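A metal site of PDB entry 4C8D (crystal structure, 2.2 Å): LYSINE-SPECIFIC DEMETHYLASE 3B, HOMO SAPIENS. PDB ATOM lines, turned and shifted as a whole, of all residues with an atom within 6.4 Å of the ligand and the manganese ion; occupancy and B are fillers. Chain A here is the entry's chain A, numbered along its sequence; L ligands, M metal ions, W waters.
The manganese ion is bound by water W3, at 1.7 Å. NE2 of His 311 binds the manganese ion (2.0 Å). The manganese ion is bound by an oxygen (O2) of the ligand (2.1 Å). A ring nitrogen (NE2) of His 182 binds the manganese ion, 2.2 Å away. The manganese ion is bound by the side-chain carboxylate (OD2) of Asp 184, 2.3 Å away. O3 of the ligand binds the manganese ion, 2.3 Å away.
Tyr 163 touches the ligand (CB to O4, 3.5 Å). CH2 of Trp 236 touches O1 of the ligand (3.6 Å). CD1 of Ile 305 touches O1 of the ligand, 3.6 Å away. CG2 of Val 313 touches C3 of the ligand (3.5 Å). Hydrophobic or aromatic side chains that line the ligand: Tyr 163, His 182, Trp 236, Ile 305, His 311 and Val 313. Within 4 Å of the ligand: Tyr 163, Thr 179, His 182, Asp 184, Asn 190, Trp 236, Ile 305, His 311, Val 313 and Lys 321. The nearest printed residue that does not touch the ligand is Thr 178 (4.02 Å).
Water W3 lies within hydrogen-bond range of OH of Tyr 163 and OD1 of Asp 184. Water W2 lies within hydrogen-bond range of O5 of the ligand (2.7 Å) and NZ of Lys 321 (3.4 Å).
Three residues have an atom within 4 Å of the manganese ion: His 182, Asp 184 and His 311. The nearest printed residue that does not touch the manganese ion is Tyr 163 (4.4 Å).
The side-chain amide nitrogen of Asn 190 lies within hydrogen-bond range of an oxygen (O1) of the ligand (2.9 Å). The side-chain amino group (NZ) of Lys 321 lies within salt-bridge range of an oxygen (O4) of the ligand. OG1 of Thr 179 is in hydrogen-bond range of O5 of the ligand (2.5 Å).
The backbone NH (N) of Thr 179 lies within hydrogen-bond range of the backbone carbonyl oxygen (O) of Val 313, 2.9 Å away. OE1 of Gln 297 is in hydrogen-bond range of NE1 of Trp 236, 2.7 Å away. The backbone carbonyl oxygen (O) of Lys 321 sits at hydrogen-bond distance from the backbone NH (N) of Tyr 163 (2.8 Å). O of Val 313 sits at hydrogen-bond distance from N of Thr 178 (2.9 Å). The backbone NH (N) of Ile 305 is in hydrogen-bond range of the backbone carbonyl oxygen (O) of Ala 188 (3.0 Å). The backbone carbonyl oxygen (O) of Asn 190 lies within hydrogen-bond range of the backbone NH (N) of Val 303, 2.8 Å away. The backbone carbonyl oxygen (O) of Asn 190 sits at hydrogen-bond distance from the side-chain amide nitrogen (NE2) of Gln 297. OD1 of Asn 315 is in hydrogen-bond range of NZ of Lys 321, at 3.0 Å.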
ATOM      1  N   LYS A 106      31.465  19.995 -34.300  1.00  0.00           N
ATOM      2  CA  LYS A 106      30.410  19.552 -33.411  1.00  0.00           C
ATOM      3  C   LYS A 106      29.423  18.704 -34.233  1.00  0.00           C
ATOM      4  O   LYS A 106      29.111  19.030 -35.377  1.00  0.00           O
ATOM      5  CB  LYS A 106      29.732  20.777 -32.775  1.00  0.00           C
ATOM      6  CG  LYS A 106      28.261  20.622 -32.425  1.00  0.00           C
ATOM      7  CD  LYS A 106      27.797  21.675 -31.430  1.00  0.00           C
ATOM      8  CE  LYS A 106      27.847  23.082 -31.981  1.00  0.00           C
ATOM      9  NZ  LYS A 106      27.442  24.069 -30.952  1.00  0.00           N
ATOM     10  N   TYR A 163      25.729  16.034 -26.311  1.00  0.00           N
ATOM     11  CA  TYR A 163      26.537  17.127 -26.817  1.00  0.00           C
ATOM     12  C   TYR A 163      27.929  16.578 -27.057  1.00  0.00           C
ATOM     13  O   TYR A 163      28.682  16.301 -26.107  1.00  0.00           O
ATOM     14  CB  TYR A 163      26.570  18.292 -25.831  1.00  0.00           C
ATOM     15  CG  TYR A 163      25.212  18.820 -25.467  1.00  0.00           C
ATOM     16  CD1 TYR A 163      24.472  18.243 -24.419  1.00  0.00           C
ATOM     17  CD2 TYR A 163      24.653  19.886 -26.157  1.00  0.00           C
ATOM     18  CE1 TYR A 163      23.218  18.722 -24.092  1.00  0.00           C
ATOM     19  CE2 TYR A 163      23.393  20.370 -25.837  1.00  0.00           C
ATOM     20  CZ  TYR A 163      22.675  19.789 -24.811  1.00  0.00           C
ATOM     21  OH  TYR A 163      21.430  20.312 -24.489  1.00  0.00           O
ATOM     22  N   ASN A 164      28.247  16.403 -28.322  1.00  0.00           N
ATOM     23  CA  ASN A 164      29.499  15.837 -28.748  1.00  0.00           C
ATOM     24  C   ASN A 164      30.219  16.849 -29.647  1.00  0.00           C
ATOM     25  O   ASN A 164      29.677  17.251 -30.668  1.00  0.00           O
ATOM     26  CB  ASN A 164      29.246  14.550 -29.513  1.00  0.00           C
ATOM     27  CG  ASN A 164      28.413  13.574 -28.734  1.00  0.00           C
ATOM     28  OD1 ASN A 164      28.719  13.240 -27.589  1.00  0.00           O
ATOM     29  ND2 ASN A 164      27.356  13.098 -29.366  1.00  0.00           N
ATOM     30  N   ALA A 165      31.409  17.271 -29.238  1.00  0.00           N
ATOM     31  CA  ALA A 165      32.202  18.203 -30.048  1.00  0.00           C
ATOM     32  C   ALA A 165      33.659  18.144 -29.655  1.00  0.00           C
ATOM     33  O   ALA A 165      33.988  17.712 -28.548  1.00  0.00           O
ATOM     34  CB  ALA A 165      31.672  19.624 -29.901  1.00  0.00           C
ATOM     35  N   THR A 178      31.879  26.689 -27.891  1.00  0.00           N
ATOM     36  CA  THR A 178      31.412  25.391 -28.398  1.00  0.00           C
ATOM     37  C   THR A 178      29.887  25.500 -28.535  1.00  0.00           C
ATOM     38  O   THR A 178      29.323  25.208 -29.597  1.00  0.00           O
ATOM     39  CB  THR A 178      31.794  24.256 -27.435  1.00  0.00           C
ATOM     40  OG1 THR A 178      33.219  24.196 -27.311  1.00  0.00           O
ATOM     41  CG2 THR A 178      31.239  22.929 -27.919  1.00  0.00           C
ATOM     42  N   THR A 179      29.235  25.932 -27.454  1.00  0.00           N
ATOM     43  CA  THR A 179      27.811  26.254 -27.493  1.00  0.00           C
ATOM     44  C   THR A 179      27.628  27.663 -26.946  1.00  0.00           C
ATOM     45  O   THR A 179      28.044  27.961 -25.827  1.00  0.00           O
ATOM     46  CB  THR A 179      27.003  25.229 -26.683  1.00  0.00           C
ATOM     47  OG1 THR A 179      27.372  23.919 -27.097  1.00  0.00           O
ATOM     48  CG2 THR A 179      25.499  25.415 -26.900  1.00  0.00           C
ATOM     49  N   ASN A 180      27.050  28.538 -27.757  1.00  0.00           N
ATOM     50  CA  ASN A 180      26.826  29.922 -27.365  1.00  0.00           C
ATOM     51  C   ASN A 180      25.814  30.094 -26.237  1.00  0.00           C
ATOM     52  O   ASN A 180      24.965  29.219 -26.003  1.00  0.00           O
ATOM     53  CB  ASN A 180      26.338  30.746 -28.547  1.00  0.00           C
ATOM     54  CG  ASN A 180      27.439  31.099 -29.503  1.00  0.00           C
ATOM     55  OD1 ASN A 180      28.612  31.075 -29.157  1.00  0.00           O
ATOM     56  ND2 ASN A 180      27.053  31.426 -30.722  1.00  0.00           N
ATOM     57  N   HIS A 182      22.825  30.671 -24.078  1.00  0.00           N
ATOM     58  CA  HIS A 182      21.397  30.485 -24.257  1.00  0.00           C
ATOM     59  C   HIS A 182      20.802  30.024 -22.916  1.00  0.00           C
ATOM     60  O   HIS A 182      21.530  29.885 -21.925  1.00  0.00           O
ATOM     61  CB  HIS A 182      21.143  29.421 -25.310  1.00  0.00           C
ATOM     62  CG  HIS A 182      21.522  28.056 -24.841  1.00  0.00           C
ATOM     63  ND1 HIS A 182      22.822  27.700 -24.563  1.00  0.00           N
ATOM     64  CD2 HIS A 182      20.766  26.967 -24.564  1.00  0.00           C
ATOM     65  CE1 HIS A 182      22.859  26.448 -24.154  1.00  0.00           C
ATOM     66  NE2 HIS A 182      21.624  25.982 -24.152  1.00  0.00           N
ATOM     67  N   LEU A 183      19.501  29.774 -22.901  1.00  0.00           N
ATOM     68  CA  LEU A 183      18.872  29.137 -21.749  1.00  0.00           C
ATOM     69  C   LEU A 183      18.014  27.978 -22.219  1.00  0.00           C
ATOM     70  O   LEU A 183      17.643  27.933 -23.376  1.00  0.00           O
ATOM     71  CB  LEU A 183      18.043  30.143 -20.953  1.00  0.00           C
ATOM     72  CG  LEU A 183      16.912  30.898 -21.669  1.00  0.00           C
ATOM     73  CD1 LEU A 183      15.733  30.000 -22.003  1.00  0.00           C
ATOM     74  CD2 LEU A 183      16.445  32.064 -20.800  1.00  0.00           C
ATOM     75  N   ASP A 184      17.693  27.058 -21.317  1.00  0.00           N
ATOM     76  CA  ASP A 184      16.737  25.992 -21.626  1.00  0.00           C
ATOM     77  C   ASP A 184      15.511  26.121 -20.732  1.00  0.00           C
ATOM     78  O   ASP A 184      15.546  26.793 -19.693  1.00  0.00           O
ATOM     79  CB  ASP A 184      17.395  24.597 -21.507  1.00  0.00           C
ATOM     80  CG  ASP A 184      18.419  24.346 -22.599  1.00  0.00           C
ATOM     81  OD1 ASP A 184      18.043  24.080 -23.760  1.00  0.00           O
ATOM     82  OD2 ASP A 184      19.621  24.419 -22.311  1.00  0.00           O
ATOM     83  N   ALA A 188      17.888  20.591 -16.091  1.00  0.00           N
ATOM     84  CA  ALA A 188      18.655  19.500 -16.712  1.00  0.00           C
ATOM     85  C   ALA A 188      19.870  19.145 -15.891  1.00  0.00           C
ATOM     86  O   ALA A 188      20.336  19.954 -15.075  1.00  0.00           O
ATOM     87  CB  ALA A 188      19.094  19.874 -18.110  1.00  0.00           C
ATOM     88  N   VAL A 189      20.358  17.922 -16.091  1.00  0.00           N
ATOM     89  CA  VAL A 189      21.664  17.513 -15.612  1.00  0.00           C
ATOM     90  C   VAL A 189      22.495  17.063 -16.803  1.00  0.00           C
ATOM     91  O   VAL A 189      22.058  16.241 -17.607  1.00  0.00           O
ATOM     92  CB  VAL A 189      21.592  16.410 -14.517  1.00  0.00           C
ATOM     93  CG1 VAL A 189      20.831  15.181 -15.004  1.00  0.00           C
ATOM     94  CG2 VAL A 189      22.994  16.038 -14.061  1.00  0.00           C
ATOM     95  N   ASN A 190      23.703  17.622 -16.924  1.00  0.00           N
ATOM     96  CA  ASN A 190      24.596  17.341 -18.034  1.00  0.00           C
ATOM     97  C   ASN A 190      25.805  16.617 -17.505  1.00  0.00           C
ATOM     98  O   ASN A 190      26.558  17.152 -16.696  1.00  0.00           O
ATOM     99  CB  ASN A 190      25.025  18.648 -18.703  1.00  0.00           C
ATOM    100  CG  ASN A 190      26.023  18.434 -19.806  1.00  0.00           C
ATOM    101  OD1 ASN A 190      27.095  17.854 -19.585  1.00  0.00           O
ATOM    102  ND2 ASN A 190      25.692  18.899 -21.010  1.00  0.00           N
ATOM    103  N   ALA A 234      35.333  20.643 -20.269  1.00  0.00           N
ATOM    104  CA  ALA A 234      34.729  21.862 -20.796  1.00  0.00           C
ATOM    105  C   ALA A 234      34.661  22.967 -19.752  1.00  0.00           C
ATOM    106  O   ALA A 234      34.609  22.689 -18.558  1.00  0.00           O
ATOM    107  CB  ALA A 234      33.339  21.565 -21.348  1.00  0.00           C
ATOM    108  N   TRP A 236      32.389  26.081 -18.541  1.00  0.00           N
ATOM    109  CA  TRP A 236      31.045  26.611 -18.546  1.00  0.00           C
ATOM    110  C   TRP A 236      31.013  27.964 -17.897  1.00  0.00           C
ATOM    111  O   TRP A 236      31.707  28.199 -16.904  1.00  0.00           O
ATOM    112  CB  TRP A 236      30.127  25.733 -17.691  1.00  0.00           C
ATOM    113  CG  TRP A 236      29.811  24.385 -18.231  1.00  0.00           C
ATOM    114  CD1 TRP A 236      30.667  23.331 -18.371  1.00  0.00           C
ATOM    115  CD2 TRP A 236      28.528  23.925 -18.666  1.00  0.00           C
ATOM    116  NE1 TRP A 236      30.006  22.255 -18.886  1.00  0.00           N
ATOM    117  CE2 TRP A 236      28.691  22.594 -19.086  1.00  0.00           C
ATOM    118  CE3 TRP A 236      27.268  24.517 -18.742  1.00  0.00           C
ATOM    119  CZ2 TRP A 236      27.626  21.828 -19.571  1.00  0.00           C
ATOM    120  CZ3 TRP A 236      26.209  23.759 -19.241  1.00  0.00           C
ATOM    121  CH2 TRP A 236      26.396  22.433 -19.647  1.00  0.00           C
ATOM    122  N   GLN A 297      34.109  21.509 -16.149  1.00  0.00           N
ATOM    123  CA  GLN A 297      33.496  20.196 -16.039  1.00  0.00           C
ATOM    124  C   GLN A 297      34.517  19.127 -16.416  1.00  0.00           C
ATOM    125  O   GLN A 297      34.898  19.000 -17.588  1.00  0.00           O
ATOM    126  CB  GLN A 297      32.272  20.140 -16.950  1.00  0.00           C
ATOM    127  CG  GLN A 297      31.452  18.861 -16.863  1.00  0.00           C
ATOM    128  CD  GLN A 297      30.281  18.853 -17.829  1.00  0.00           C
ATOM    129  OE1 GLN A 297      30.287  19.574 -18.844  1.00  0.00           O
ATOM    130  NE2 GLN A 297      29.263  18.042 -17.517  1.00  0.00           N
ATOM    131  N   VAL A 303      26.697  18.502 -14.252  1.00  0.00           N
ATOM    132  CA  VAL A 303      26.342  19.873 -14.018  1.00  0.00           C
ATOM    133  C   VAL A 303      24.813  20.008 -14.054  1.00  0.00           C
ATOM    134  O   VAL A 303      24.192  19.697 -15.064  1.00  0.00           O
ATOM    135  CB  VAL A 303      26.966  20.776 -15.092  1.00  0.00           C
ATOM    136  CG1 VAL A 303      26.515  22.219 -14.919  1.00  0.00           C
ATOM    137  CG2 VAL A 303      28.472  20.647 -15.048  1.00  0.00           C
ATOM    138  N   ILE A 305      21.756  22.398 -14.211  1.00  0.00           N
ATOM    139  CA  ILE A 305      21.506  23.708 -14.790  1.00  0.00           C
ATOM    140  C   ILE A 305      20.044  24.013 -14.545  1.00  0.00           C
ATOM    141  O   ILE A 305      19.174  23.290 -15.057  1.00  0.00           O
ATOM    142  CB  ILE A 305      21.737  23.685 -16.323  1.00  0.00           C
ATOM    143  CG1 ILE A 305      23.077  23.013 -16.662  1.00  0.00           C
ATOM    144  CG2 ILE A 305      21.628  25.085 -16.909  1.00  0.00           C
ATOM    145  CD1 ILE A 305      23.062  22.241 -17.973  1.00  0.00           C
ATOM    146  N   HIS A 311      23.400  30.005 -19.976  1.00  0.00           N
ATOM    147  CA  HIS A 311      24.672  29.313 -19.944  1.00  0.00           C
ATOM    148  C   HIS A 311      25.306  29.172 -21.322  1.00  0.00           C
ATOM    149  O   HIS A 311      24.605  29.116 -22.336  1.00  0.00           O
ATOM    150  CB  HIS A 311      24.512  27.930 -19.294  1.00  0.00           C
ATOM    151  CG  HIS A 311      23.528  27.035 -19.985  1.00  0.00           C
ATOM    152  ND1 HIS A 311      22.168  27.147 -19.782  1.00  0.00           N
ATOM    153  CD2 HIS A 311      23.701  26.004 -20.843  1.00  0.00           C
ATOM    154  CE1 HIS A 311      21.541  26.236 -20.506  1.00  0.00           C
ATOM    155  NE2 HIS A 311      22.448  25.541 -21.167  1.00  0.00           N
ATOM    156  N   GLN A 312      26.643  29.099 -21.300  1.00  0.00           N
ATOM    157  CA  GLN A 312      27.468  28.891 -22.479  1.00  0.00           C
ATOM    158  C   GLN A 312      28.531  27.838 -22.147  1.00  0.00           C
ATOM    159  O   GLN A 312      28.955  27.706 -20.992  1.00  0.00           O
ATOM    160  CB  GLN A 312      28.127  30.203 -22.911  1.00  0.00           C
ATOM    161  CG  GLN A 312      29.047  30.822 -21.855  1.00  0.00           C
ATOM    162  CD  GLN A 312      29.623  32.178 -22.272  1.00  0.00           C
ATOM    163  OE1 GLN A 312      29.036  32.890 -23.082  1.00  0.00           O
ATOM    164  NE2 GLN A 312      30.765  32.545 -21.709  1.00  0.00           N
ATOM    165  N   VAL A 313      28.979  27.119 -23.185  1.00  0.00           N
ATOM    166  CA  VAL A 313      29.975  26.063 -22.998  1.00  0.00           C
ATOM    167  C   VAL A 313      31.132  26.184 -24.003  1.00  0.00           C
ATOM    168  O   VAL A 313      30.936  26.530 -25.174  1.00  0.00           O
ATOM    169  CB  VAL A 313      29.319  24.663 -23.092  1.00  0.00           C
ATOM    170  CG1 VAL A 313      30.317  23.573 -22.716  1.00  0.00           C
ATOM    171  CG2 VAL A 313      28.062  24.607 -22.211  1.00  0.00           C
ATOM    172  N   HIS A 314      32.337  25.916 -23.508  1.00  0.00           N
ATOM    173  CA  HIS A 314      33.546  26.023 -24.290  1.00  0.00           C
ATOM    174  C   HIS A 314      34.380  24.786 -23.997  1.00  0.00           C
ATOM    175  O   HIS A 314      35.034  24.696 -22.949  1.00  0.00           O
ATOM    176  CB  HIS A 314      34.301  27.299 -23.884  1.00  0.00           C
ATOM    177  CG  HIS A 314      35.619  27.454 -24.569  1.00  0.00           C
ATOM    178  ND1 HIS A 314      35.808  28.309 -25.639  1.00  0.00           N
ATOM    179  CD2 HIS A 314      36.818  26.870 -24.354  1.00  0.00           C
ATOM    180  CE1 HIS A 314      37.063  28.243 -26.039  1.00  0.00           C
ATOM    181  NE2 HIS A 314      37.697  27.374 -25.273  1.00  0.00           N
ATOM    182  N   ASN A 315      34.348  23.843 -24.930  1.00  0.00           N
ATOM    183  CA  ASN A 315      35.091  22.612 -24.802  1.00  0.00           C
ATOM    184  C   ASN A 315      36.560  22.890 -24.865  1.00  0.00           C
ATOM    185  O   ASN A 315      37.016  23.665 -25.720  1.00  0.00           O
ATOM    186  CB  ASN A 315      34.743  21.617 -25.887  1.00  0.00           C
ATOM    187  CG  ASN A 315      33.366  21.017 -25.711  1.00  0.00           C
ATOM    188  OD1 ASN A 315      32.584  21.478 -24.897  1.00  0.00           O
ATOM    189  ND2 ASN A 315      33.089  19.962 -26.471  1.00  0.00           N
ATOM    190  N   LYS A 321      29.190  14.467 -23.885  1.00  0.00           N
ATOM    191  CA  LYS A 321      28.277  14.860 -22.822  1.00  0.00           C
ATOM    192  C   LYS A 321      26.888  14.301 -23.119  1.00  0.00           C
ATOM    193  O   LYS A 321      26.423  14.311 -24.274  1.00  0.00           O
ATOM    194  CB  LYS A 321      28.185  16.378 -22.689  1.00  0.00           C
ATOM    195  CG  LYS A 321      29.512  17.116 -22.553  1.00  0.00           C
ATOM    196  CD  LYS A 321      29.273  18.551 -22.122  1.00  0.00           C
ATOM    197  CE  LYS A 321      30.398  19.497 -22.513  1.00  0.00           C
ATOM    198  NZ  LYS A 321      30.207  19.967 -23.915  1.00  0.00           N
ATOM    199  N   ALA A 323      22.918  14.754 -21.468  1.00  0.00           N
ATOM    200  CA  ALA A 323      22.078  15.513 -20.550  1.00  0.00           C
ATOM    201  C   ALA A 323      20.663  14.921 -20.429  1.00  0.00           C
ATOM    202  O   ALA A 323      20.092  14.461 -21.432  1.00  0.00           O
ATOM    203  CB  ALA A 323      21.982  16.962 -20.983  1.00  0.00           C
HETATM  204  C1  LIG L   1      23.284  21.878 -21.876  1.00  0.00           C
HETATM  205  C2  LIG L   1      24.210  22.475 -22.840  1.00  0.00           C
HETATM  206  C3  LIG L   1      26.133  22.530 -24.264  1.00  0.00           C
HETATM  207  C4  LIG L   1      27.397  21.778 -24.585  1.00  0.00           C
HETATM  208  O1  LIG L   1      23.573  20.862 -21.219  1.00  0.00           O
HETATM  209  O2  LIG L   1      22.183  22.443 -21.756  1.00  0.00           O
HETATM  210  O3  LIG L   1      23.858  23.502 -23.401  1.00  0.00           O
HETATM  211  O4  LIG L   1      27.729  20.853 -23.830  1.00  0.00           O
HETATM  212  N1  LIG L   1      25.384  21.946 -23.166  1.00  0.00           N
HETATM  213  O5  LIG L   1      28.062  22.101 -25.600  1.00  0.00           O
HETATM  214 MN    MN M   1      21.859  24.333 -22.662  1.00  0.00          MN
HETATM  215  O   HOH W   1      19.630  22.447 -20.054  1.00  0.00           O
HETATM  216  O   HOH W   2      29.141  20.204 -27.146  1.00  0.00           O
HETATM  217  O   HOH W   3      21.165  23.420 -23.936  1.00  0.00           O
HETATM  218  O   HOH W   4      21.212  20.025 -20.254  1.00  0.00           O
